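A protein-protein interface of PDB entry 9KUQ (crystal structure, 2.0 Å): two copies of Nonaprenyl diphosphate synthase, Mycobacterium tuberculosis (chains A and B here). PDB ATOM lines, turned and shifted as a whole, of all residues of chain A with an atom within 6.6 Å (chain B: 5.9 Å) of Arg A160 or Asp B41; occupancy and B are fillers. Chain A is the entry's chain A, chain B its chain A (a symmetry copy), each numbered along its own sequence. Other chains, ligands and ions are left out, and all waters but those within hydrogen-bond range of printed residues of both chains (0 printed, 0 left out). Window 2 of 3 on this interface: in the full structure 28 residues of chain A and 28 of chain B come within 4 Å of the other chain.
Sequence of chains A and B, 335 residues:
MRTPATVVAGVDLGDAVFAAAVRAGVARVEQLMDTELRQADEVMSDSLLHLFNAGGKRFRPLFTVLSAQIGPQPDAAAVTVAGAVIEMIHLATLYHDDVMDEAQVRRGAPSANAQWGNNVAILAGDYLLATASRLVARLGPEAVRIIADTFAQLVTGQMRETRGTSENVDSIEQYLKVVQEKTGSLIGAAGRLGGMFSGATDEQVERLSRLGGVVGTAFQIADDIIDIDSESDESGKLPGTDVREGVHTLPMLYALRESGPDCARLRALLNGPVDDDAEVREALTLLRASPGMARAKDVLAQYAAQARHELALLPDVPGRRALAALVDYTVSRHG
SD of Met A159 sits close to the backbone carbonyl oxygen (O) of Val B43 (3.3 Å).
The side-chain carboxylate (OD2) of Asp B41 is in salt-bridge range of the guanidinium group (NH2) of Arg A160 (3.1 Å).
SD of Met A159 is bonded to SD of Met B44, at 2.0 Å.
N of Val B43 lies close to OD1 of Asp B41 (3.1 Å).
NE of Arg A163 lies close to OE1 of Gln A174 (3.4 Å).
The guanidinium group of Arg A160 is in salt-bridge range of the side-chain carboxylate of Glu A181 (2.6 Å).
CG1 of Val A155 touches SD of Met B44 (3.96 Å).
CD1 of Tyr B127 touches CG1 of Val A155 (3.6 Å).
Asp B41 touches Thr A156 (CB to CG2, 3.3 Å).
Tyr B127 touches Thr A156 (CE1 to OG1, 3.7 Å).
CA of Arg A160 touches CG1 of Val B43, 3.4 Å away.
Val B43 touches Arg A163.
Of the printed residues of chain B, Arg A160 touches Asp B41 and Val B43.
Of chain A, only Thr A156 and Arg A160 come within 4 Å of Asp B41.
Printed residues of chain B within 4 Å of Thr A156: Asp B41 (3.3 Å) and Tyr B127 (3.7 Å).
Of the printed residues of chain A, Val B43 touches Met A159 (3.0 Å), Arg A160 (3.4 Å) and Arg A163 (3.7 Å).
Printed residues of chain B within 4 Å of Val A155: Met B44 and Tyr B127.
Of the printed residues of chain A, Met B44 touches Val A155 (3.96 Å) and Met A159 (2.0 Å).
Of the 15 printed residues of chain A, 5 touch a printed residue of chain B.
Of the 8 printed residues of chain B, 4 touch a printed residue of chain A.
Hydrophobic or aromatic side chains of chain B within 4 Å of the printed part of chain A: Val B43, Met B44 and Tyr B127.
Along chain B the printed residues that touch a printed residue of chain A span positions 41 to 127.
Among the printed residues, 9 pairs touch across the chains.
Among the printed residues, Asp or Glu carboxylates within 4 Å of a Lys or Arg side-chain nitrogen of the other chain: Arg A160 with Asp B41.
No position is printed for both chains.
Of the 9 pairs that touch across the chains among the printed residues, none has its exchanged pair printed and touching as well.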
ATOM      1  N   VAL A 155      -9.349  21.936  18.376  1.00  0.00           N
ATOM      2  CA  VAL A 155     -10.051  22.098  19.666  1.00  0.00           C
ATOM      3  C   VAL A 155     -10.039  23.589  20.006  1.00  0.00           C
ATOM      4  O   VAL A 155     -11.149  24.176  20.087  1.00  0.00           O
ATOM      5  CB  VAL A 155      -9.377  21.214  20.729  1.00  0.00           C
ATOM      6  CG1 VAL A 155      -9.782  21.592  22.143  1.00  0.00           C
ATOM      7  CG2 VAL A 155      -9.643  19.731  20.449  1.00  0.00           C
ATOM      8  N   THR A 156      -8.842  24.167  20.179  1.00  0.00           N
ATOM      9  CA  THR A 156      -8.604  25.596  20.525  1.00  0.00           C
ATOM     10  C   THR A 156      -9.539  26.504  19.733  1.00  0.00           C
ATOM     11  O   THR A 156      -9.941  27.514  20.279  1.00  0.00           O
ATOM     12  CB  THR A 156      -7.169  26.010  20.216  1.00  0.00           C
ATOM     13  OG1 THR A 156      -6.314  25.034  20.796  1.00  0.00           O
ATOM     14  CG2 THR A 156      -6.844  27.385  20.738  1.00  0.00           C
ATOM     15  N   GLY A 157      -9.801  26.157  18.477  1.00  0.00           N
ATOM     16  CA  GLY A 157     -10.689  26.877  17.547  1.00  0.00           C
ATOM     17  C   GLY A 157     -12.164  26.785  17.916  1.00  0.00           C
ATOM     18  O   GLY A 157     -12.811  27.833  17.987  1.00  0.00           O
ATOM     19  N   GLN A 158     -12.706  25.574  18.050  1.00  0.00           N
ATOM     20  CA  GLN A 158     -14.070  25.345  18.604  1.00  0.00           C
ATOM     21  C   GLN A 158     -14.148  26.053  19.969  1.00  0.00           C
ATOM     22  O   GLN A 158     -15.129  26.796  20.209  1.00  0.00           O
ATOM     23  CB  GLN A 158     -14.363  23.844  18.733  1.00  0.00           C
ATOM     24  CG  GLN A 158     -14.573  23.118  17.405  1.00  0.00           C
ATOM     25  CD  GLN A 158     -14.452  21.618  17.565  1.00  0.00           C
ATOM     26  OE1 GLN A 158     -15.384  20.870  17.300  1.00  0.00           O
ATOM     27  NE2 GLN A 158     -13.301  21.154  18.024  1.00  0.00           N
ATOM     28  N   MET A 159     -13.132  25.833  20.808  1.00  0.00           N
ATOM     29  CA  MET A 159     -12.927  26.444  22.148  1.00  0.00           C
ATOM     30  C   MET A 159     -13.051  27.972  22.144  1.00  0.00           C
ATOM     31  O   MET A 159     -13.636  28.551  23.088  1.00  0.00           O
ATOM     32  CB  MET A 159     -11.499  26.133  22.568  1.00  0.00           C
ATOM     33  CG  MET A 159     -11.095  26.779  23.845  1.00  0.00           C
ATOM     34  SD  MET A 159     -10.162  25.602  24.808  1.00  0.00           S
ATOM     35  CE  MET A 159     -11.423  24.378  25.198  1.00  0.00           C
ATOM     36  N   ARG A 160     -12.368  28.613  21.204  1.00  0.00           N
ATOM     37  CA  ARG A 160     -12.275  30.086  21.089  1.00  0.00           C
ATOM     38  C   ARG A 160     -13.626  30.576  20.569  1.00  0.00           C
ATOM     39  O   ARG A 160     -14.009  31.701  20.930  1.00  0.00           O
ATOM     40  CB  ARG A 160     -11.070  30.423  20.204  1.00  0.00           C
ATOM     41  CG  ARG A 160     -10.819  31.900  19.935  1.00  0.00           C
ATOM     42  CD  ARG A 160      -9.840  32.083  18.783  1.00  0.00           C
ATOM     43  NE  ARG A 160      -8.667  31.243  18.931  1.00  0.00           N
ATOM     44  CZ  ARG A 160      -7.579  31.553  19.615  1.00  0.00           C
ATOM     45  NH1 ARG A 160      -7.476  32.730  20.203  1.00  0.00           N
ATOM     46  NH2 ARG A 160      -6.572  30.701  19.699  1.00  0.00           N
ATOM     47  N   GLU A 161     -14.319  29.752  19.775  1.00  0.00           N
ATOM     48  CA  GLU A 161     -15.711  30.007  19.300  1.00  0.00           C
ATOM     49  C   GLU A 161     -16.587  30.167  20.548  1.00  0.00           C
ATOM     50  O   GLU A 161     -17.520  30.974  20.529  1.00  0.00           O
ATOM     51  CB  GLU A 161     -16.184  28.857  18.407  1.00  0.00           C
ATOM     52  CG  GLU A 161     -17.162  29.224  17.308  1.00  0.00           C
ATOM     53  CD  GLU A 161     -17.553  28.032  16.433  1.00  0.00           C
ATOM     54  OE1 GLU A 161     -17.262  26.863  16.821  1.00  0.00           O
ATOM     55  OE2 GLU A 161     -18.123  28.257  15.353  1.00  0.00           O
ATOM     56  N   THR A 162     -16.233  29.427  21.596  1.00  0.00           N
ATOM     57  CA  THR A 162     -16.806  29.447  22.968  1.00  0.00           C
ATOM     58  C   THR A 162     -16.309  30.688  23.736  1.00  0.00           C
ATOM     59  O   THR A 162     -16.824  30.933  24.841  1.00  0.00           O
ATOM     60  CB  THR A 162     -16.458  28.105  23.637  1.00  0.00           C
ATOM     61  OG1 THR A 162     -17.595  27.246  23.567  1.00  0.00           O
ATOM     62  CG2 THR A 162     -15.986  28.216  25.070  1.00  0.00           C
ATOM     63  N   ARG A 163     -15.364  31.457  23.176  1.00  0.00           N
ATOM     64  CA  ARG A 163     -14.703  32.619  23.837  1.00  0.00           C
ATOM     65  C   ARG A 163     -14.030  32.141  25.129  1.00  0.00           C
ATOM     66  O   ARG A 163     -13.046  32.799  25.528  1.00  0.00           O
ATOM     67  CB  ARG A 163     -15.698  33.754  24.126  1.00  0.00           C
ATOM     68  CG  ARG A 163     -15.738  34.860  23.079  1.00  0.00           C
ATOM     69  CD  ARG A 163     -15.780  36.261  23.690  1.00  0.00           C
ATOM     70  NE  ARG A 163     -16.210  37.300  22.748  1.00  0.00           N
ATOM     71  CZ  ARG A 163     -16.338  38.611  23.016  1.00  0.00           C
ATOM     72  NH1 ARG A 163     -16.065  39.094  24.218  1.00  0.00           N
ATOM     73  NH2 ARG A 163     -16.740  39.441  22.069  1.00  0.00           N
ATOM     74  N   GLU A 173     -10.762  39.661  14.043  1.00  0.00           N
ATOM     75  CA  GLU A 173      -9.485  38.923  14.205  1.00  0.00           C
ATOM     76  C   GLU A 173      -9.775  37.579  14.871  1.00  0.00           C
ATOM     77  O   GLU A 173      -9.233  36.587  14.392  1.00  0.00           O
ATOM     78  CB  GLU A 173      -8.492  39.713  15.073  1.00  0.00           C
ATOM     79  CG  GLU A 173      -7.684  40.749  14.300  1.00  0.00           C
ATOM     80  CD  GLU A 173      -6.668  41.530  15.135  1.00  0.00           C
ATOM     81  OE1 GLU A 173      -5.632  40.936  15.490  1.00  0.00           O
ATOM     82  OE2 GLU A 173      -6.917  42.726  15.450  1.00  0.00           O
ATOM     83  N   GLN A 174     -10.590  37.586  15.929  1.00  0.00           N
ATOM     84  CA  GLN A 174     -10.921  36.406  16.775  1.00  0.00           C
ATOM     85  C   GLN A 174     -11.681  35.361  15.941  1.00  0.00           C
ATOM     86  O   GLN A 174     -11.351  34.165  16.060  1.00  0.00           O
ATOM     87  CB  GLN A 174     -11.701  36.790  18.049  1.00  0.00           C
ATOM     88  CG  GLN A 174     -12.514  35.632  18.648  1.00  0.00           C
ATOM     89  CD  GLN A 174     -12.806  35.682  20.134  1.00  0.00           C
ATOM     90  OE1 GLN A 174     -13.861  36.145  20.572  1.00  0.00           O
ATOM     91  NE2 GLN A 174     -11.886  35.158  20.932  1.00  0.00           N
ATOM     92  N   TYR A 175     -12.679  35.780  15.173  1.00  0.00           N
ATOM     93  CA  TYR A 175     -13.496  34.902  14.310  1.00  0.00           C
ATOM     94  C   TYR A 175     -12.538  34.213  13.329  1.00  0.00           C
ATOM     95  O   TYR A 175     -12.567  32.992  13.216  1.00  0.00           O
ATOM     96  CB  TYR A 175     -14.619  35.715  13.644  1.00  0.00           C
ATOM     97  CG  TYR A 175     -15.261  35.085  12.438  1.00  0.00           C
ATOM     98  CD1 TYR A 175     -16.324  34.204  12.545  1.00  0.00           C
ATOM     99  CD2 TYR A 175     -14.761  35.342  11.182  1.00  0.00           C
ATOM    100  CE1 TYR A 175     -16.886  33.609  11.426  1.00  0.00           C
ATOM    101  CE2 TYR A 175     -15.308  34.762  10.054  1.00  0.00           C
ATOM    102  CZ  TYR A 175     -16.385  33.905  10.167  1.00  0.00           C
ATOM    103  OH  TYR A 175     -16.911  33.377   9.014  1.00  0.00           O
ATOM    104  N   LYS A 177      -9.294  33.728  13.468  1.00  0.00           N
ATOM    105  CA  LYS A 177      -8.441  32.794  14.231  1.00  0.00           C
ATOM    106  C   LYS A 177      -9.235  31.521  14.492  1.00  0.00           C
ATOM    107  O   LYS A 177      -8.676  30.437  14.275  1.00  0.00           O
ATOM    108  CB  LYS A 177      -7.950  33.382  15.552  1.00  0.00           C
ATOM    109  CG  LYS A 177      -6.539  33.939  15.523  1.00  0.00           C
ATOM    110  CD  LYS A 177      -5.876  33.968  16.893  1.00  0.00           C
ATOM    111  CE  LYS A 177      -4.367  34.131  16.813  1.00  0.00           C
ATOM    112  NZ  LYS A 177      -3.717  32.893  16.311  1.00  0.00           N
ATOM    113  N   VAL A 178     -10.486  31.653  14.914  1.00  0.00           N
ATOM    114  CA  VAL A 178     -11.428  30.504  15.115  1.00  0.00           C
ATOM    115  C   VAL A 178     -11.450  29.651  13.839  1.00  0.00           C
ATOM    116  O   VAL A 178     -11.081  28.493  13.965  1.00  0.00           O
ATOM    117  CB  VAL A 178     -12.847  30.964  15.513  1.00  0.00           C
ATOM    118  CG1 VAL A 178     -13.922  29.943  15.151  1.00  0.00           C
ATOM    119  CG2 VAL A 178     -12.918  31.305  16.994  1.00  0.00           C
ATOM    120  N   GLU A 181      -8.403  27.740  12.976  1.00  0.00           N
ATOM    121  CA  GLU A 181      -8.086  26.675  13.946  1.00  0.00           C
ATOM    122  C   GLU A 181      -9.057  25.511  13.726  1.00  0.00           C
ATOM    123  O   GLU A 181      -8.573  24.360  13.612  1.00  0.00           O
ATOM    124  CB  GLU A 181      -8.109  27.225  15.373  1.00  0.00           C
ATOM    125  CG  GLU A 181      -6.945  28.161  15.686  1.00  0.00           C
ATOM    126  CD  GLU A 181      -6.983  28.863  17.040  1.00  0.00           C
ATOM    127  OE1 GLU A 181      -8.104  29.048  17.605  1.00  0.00           O
ATOM    128  OE2 GLU A 181      -5.892  29.182  17.548  1.00  0.00           O
ATOM    129  N   GLN B  39       1.121  25.173  28.302  1.00  0.00           N
ATOM    130  CA  GLN B  39       1.378  25.682  26.928  1.00  0.00           C
ATOM    131  C   GLN B  39       0.065  25.883  26.156  1.00  0.00           C
ATOM    132  O   GLN B  39       0.103  26.526  25.118  1.00  0.00           O
ATOM    133  CB  GLN B  39       2.289  24.737  26.162  1.00  0.00           C
ATOM    134  CG  GLN B  39       3.703  24.718  26.705  1.00  0.00           C
ATOM    135  CD  GLN B  39       4.551  23.707  25.975  1.00  0.00           C
ATOM    136  OE1 GLN B  39       4.109  23.070  25.006  1.00  0.00           O
ATOM    137  NE2 GLN B  39       5.785  23.563  26.447  1.00  0.00           N
ATOM    138  N   ALA B  40      -1.066  25.392  26.639  1.00  0.00           N
ATOM    139  CA  ALA B  40      -2.335  25.441  25.876  1.00  0.00           C
ATOM    140  C   ALA B  40      -2.785  26.899  25.732  1.00  0.00           C
ATOM    141  O   ALA B  40      -2.563  27.715  26.657  1.00  0.00           O
ATOM    142  CB  ALA B  40      -3.400  24.588  26.522  1.00  0.00           C
ATOM    143  N   ASP B  41      -3.394  27.215  24.589  1.00  0.00           N
ATOM    144  CA  ASP B  41      -3.943  28.561  24.294  1.00  0.00           C
ATOM    145  C   ASP B  41      -4.832  29.001  25.467  1.00  0.00           C
ATOM    146  O   ASP B  41      -5.567  28.154  26.019  1.00  0.00           O
ATOM    147  CB  ASP B  41      -4.722  28.570  22.979  1.00  0.00           C
ATOM    148  CG  ASP B  41      -5.113  29.971  22.555  1.00  0.00           C
ATOM    149  OD1 ASP B  41      -6.173  30.455  23.019  1.00  0.00           O
ATOM    150  OD2 ASP B  41      -4.332  30.574  21.793  1.00  0.00           O
ATOM    151  N   GLU B  42      -4.773  30.287  25.805  1.00  0.00           N
ATOM    152  CA  GLU B  42      -5.538  30.921  26.909  1.00  0.00           C
ATOM    153  C   GLU B  42      -6.966  30.362  26.925  1.00  0.00           C
ATOM    154  O   GLU B  42      -7.461  30.026  28.014  1.00  0.00           O
ATOM    155  CB  GLU B  42      -5.534  32.442  26.724  1.00  0.00           C
ATOM    156  CG  GLU B  42      -4.145  33.062  26.701  1.00  0.00           C
ATOM    157  CD  GLU B  42      -3.337  32.917  25.412  1.00  0.00           C
ATOM    158  OE1 GLU B  42      -3.149  33.943  24.706  1.00  0.00           O
ATOM    159  OE2 GLU B  42      -2.865  31.787  25.120  1.00  0.00           O
ATOM    160  N   VAL B  43      -7.616  30.230  25.765  1.00  0.00           N
ATOM    161  CA  VAL B  43      -9.084  29.942  25.714  1.00  0.00           C
ATOM    162  C   VAL B  43      -9.334  28.572  26.367  1.00  0.00           C
ATOM    163  O   VAL B  43     -10.506  28.317  26.736  1.00  0.00           O
ATOM    164  CB  VAL B  43      -9.683  30.016  24.288  1.00  0.00           C
ATOM    165  CG1 VAL B  43     -11.196  29.861  24.302  1.00  0.00           C
ATOM    166  CG2 VAL B  43      -9.337  31.313  23.574  1.00  0.00           C
ATOM    167  N   MET B  44      -8.271  27.759  26.510  1.00  0.00           N
ATOM    168  CA  MET B  44      -8.238  26.373  27.079  1.00  0.00           C
ATOM    169  C   MET B  44      -8.093  26.361  28.606  1.00  0.00           C
ATOM    170  O   MET B  44      -8.687  25.450  29.243  1.00  0.00           O
ATOM    171  CB  MET B  44      -7.030  25.605  26.528  1.00  0.00           C
ATOM    172  CG  MET B  44      -7.088  25.362  25.040  1.00  0.00           C
ATOM    173  SD  MET B  44      -8.583  24.447  24.606  1.00  0.00           S
ATOM    174  CE  MET B  44      -8.598  23.208  25.909  1.00  0.00           C
ATOM    175  N   SER B  45      -7.256  27.256  29.139  1.00  0.00           N
ATOM    176  CA  SER B  45      -6.805  27.295  30.554  1.00  0.00           C
ATOM    177  C   SER B  45      -7.951  26.902  31.514  1.00  0.00           C
ATOM    178  O   SER B  45      -7.851  25.824  32.174  1.00  0.00           O
ATOM    179  CB  SER B  45      -6.228  28.667  30.848  1.00  0.00           C
ATOM    180  OG  SER B  45      -5.717  28.727  32.168  1.00  0.00           O
ATOM    181  N   TYR B 127      -9.097  18.001  24.410  1.00  0.00           N
ATOM    182  CA  TYR B 127      -7.733  18.577  24.420  1.00  0.00           C
ATOM    183  C   TYR B 127      -6.833  17.593  25.155  1.00  0.00           C
ATOM    184  O   TYR B 127      -5.876  17.077  24.512  1.00  0.00           O
ATOM    185  CB  TYR B 127      -7.661  19.979  25.042  1.00  0.00           C
ATOM    186  CG  TYR B 127      -6.441  20.753  24.590  1.00  0.00           C
ATOM    187  CD1 TYR B 127      -6.418  21.423  23.368  1.00  0.00           C
ATOM    188  CD2 TYR B 127      -5.289  20.794  25.357  1.00  0.00           C
ATOM    189  CE1 TYR B 127      -5.298  22.121  22.922  1.00  0.00           C
ATOM    190  CE2 TYR B 127      -4.157  21.475  24.925  1.00  0.00           C
ATOM    191  CZ  TYR B 127      -4.154  22.135  23.701  1.00  0.00           C
ATOM    192  OH  TYR B 127      -3.037  22.784  23.249  1.00  0.00           O
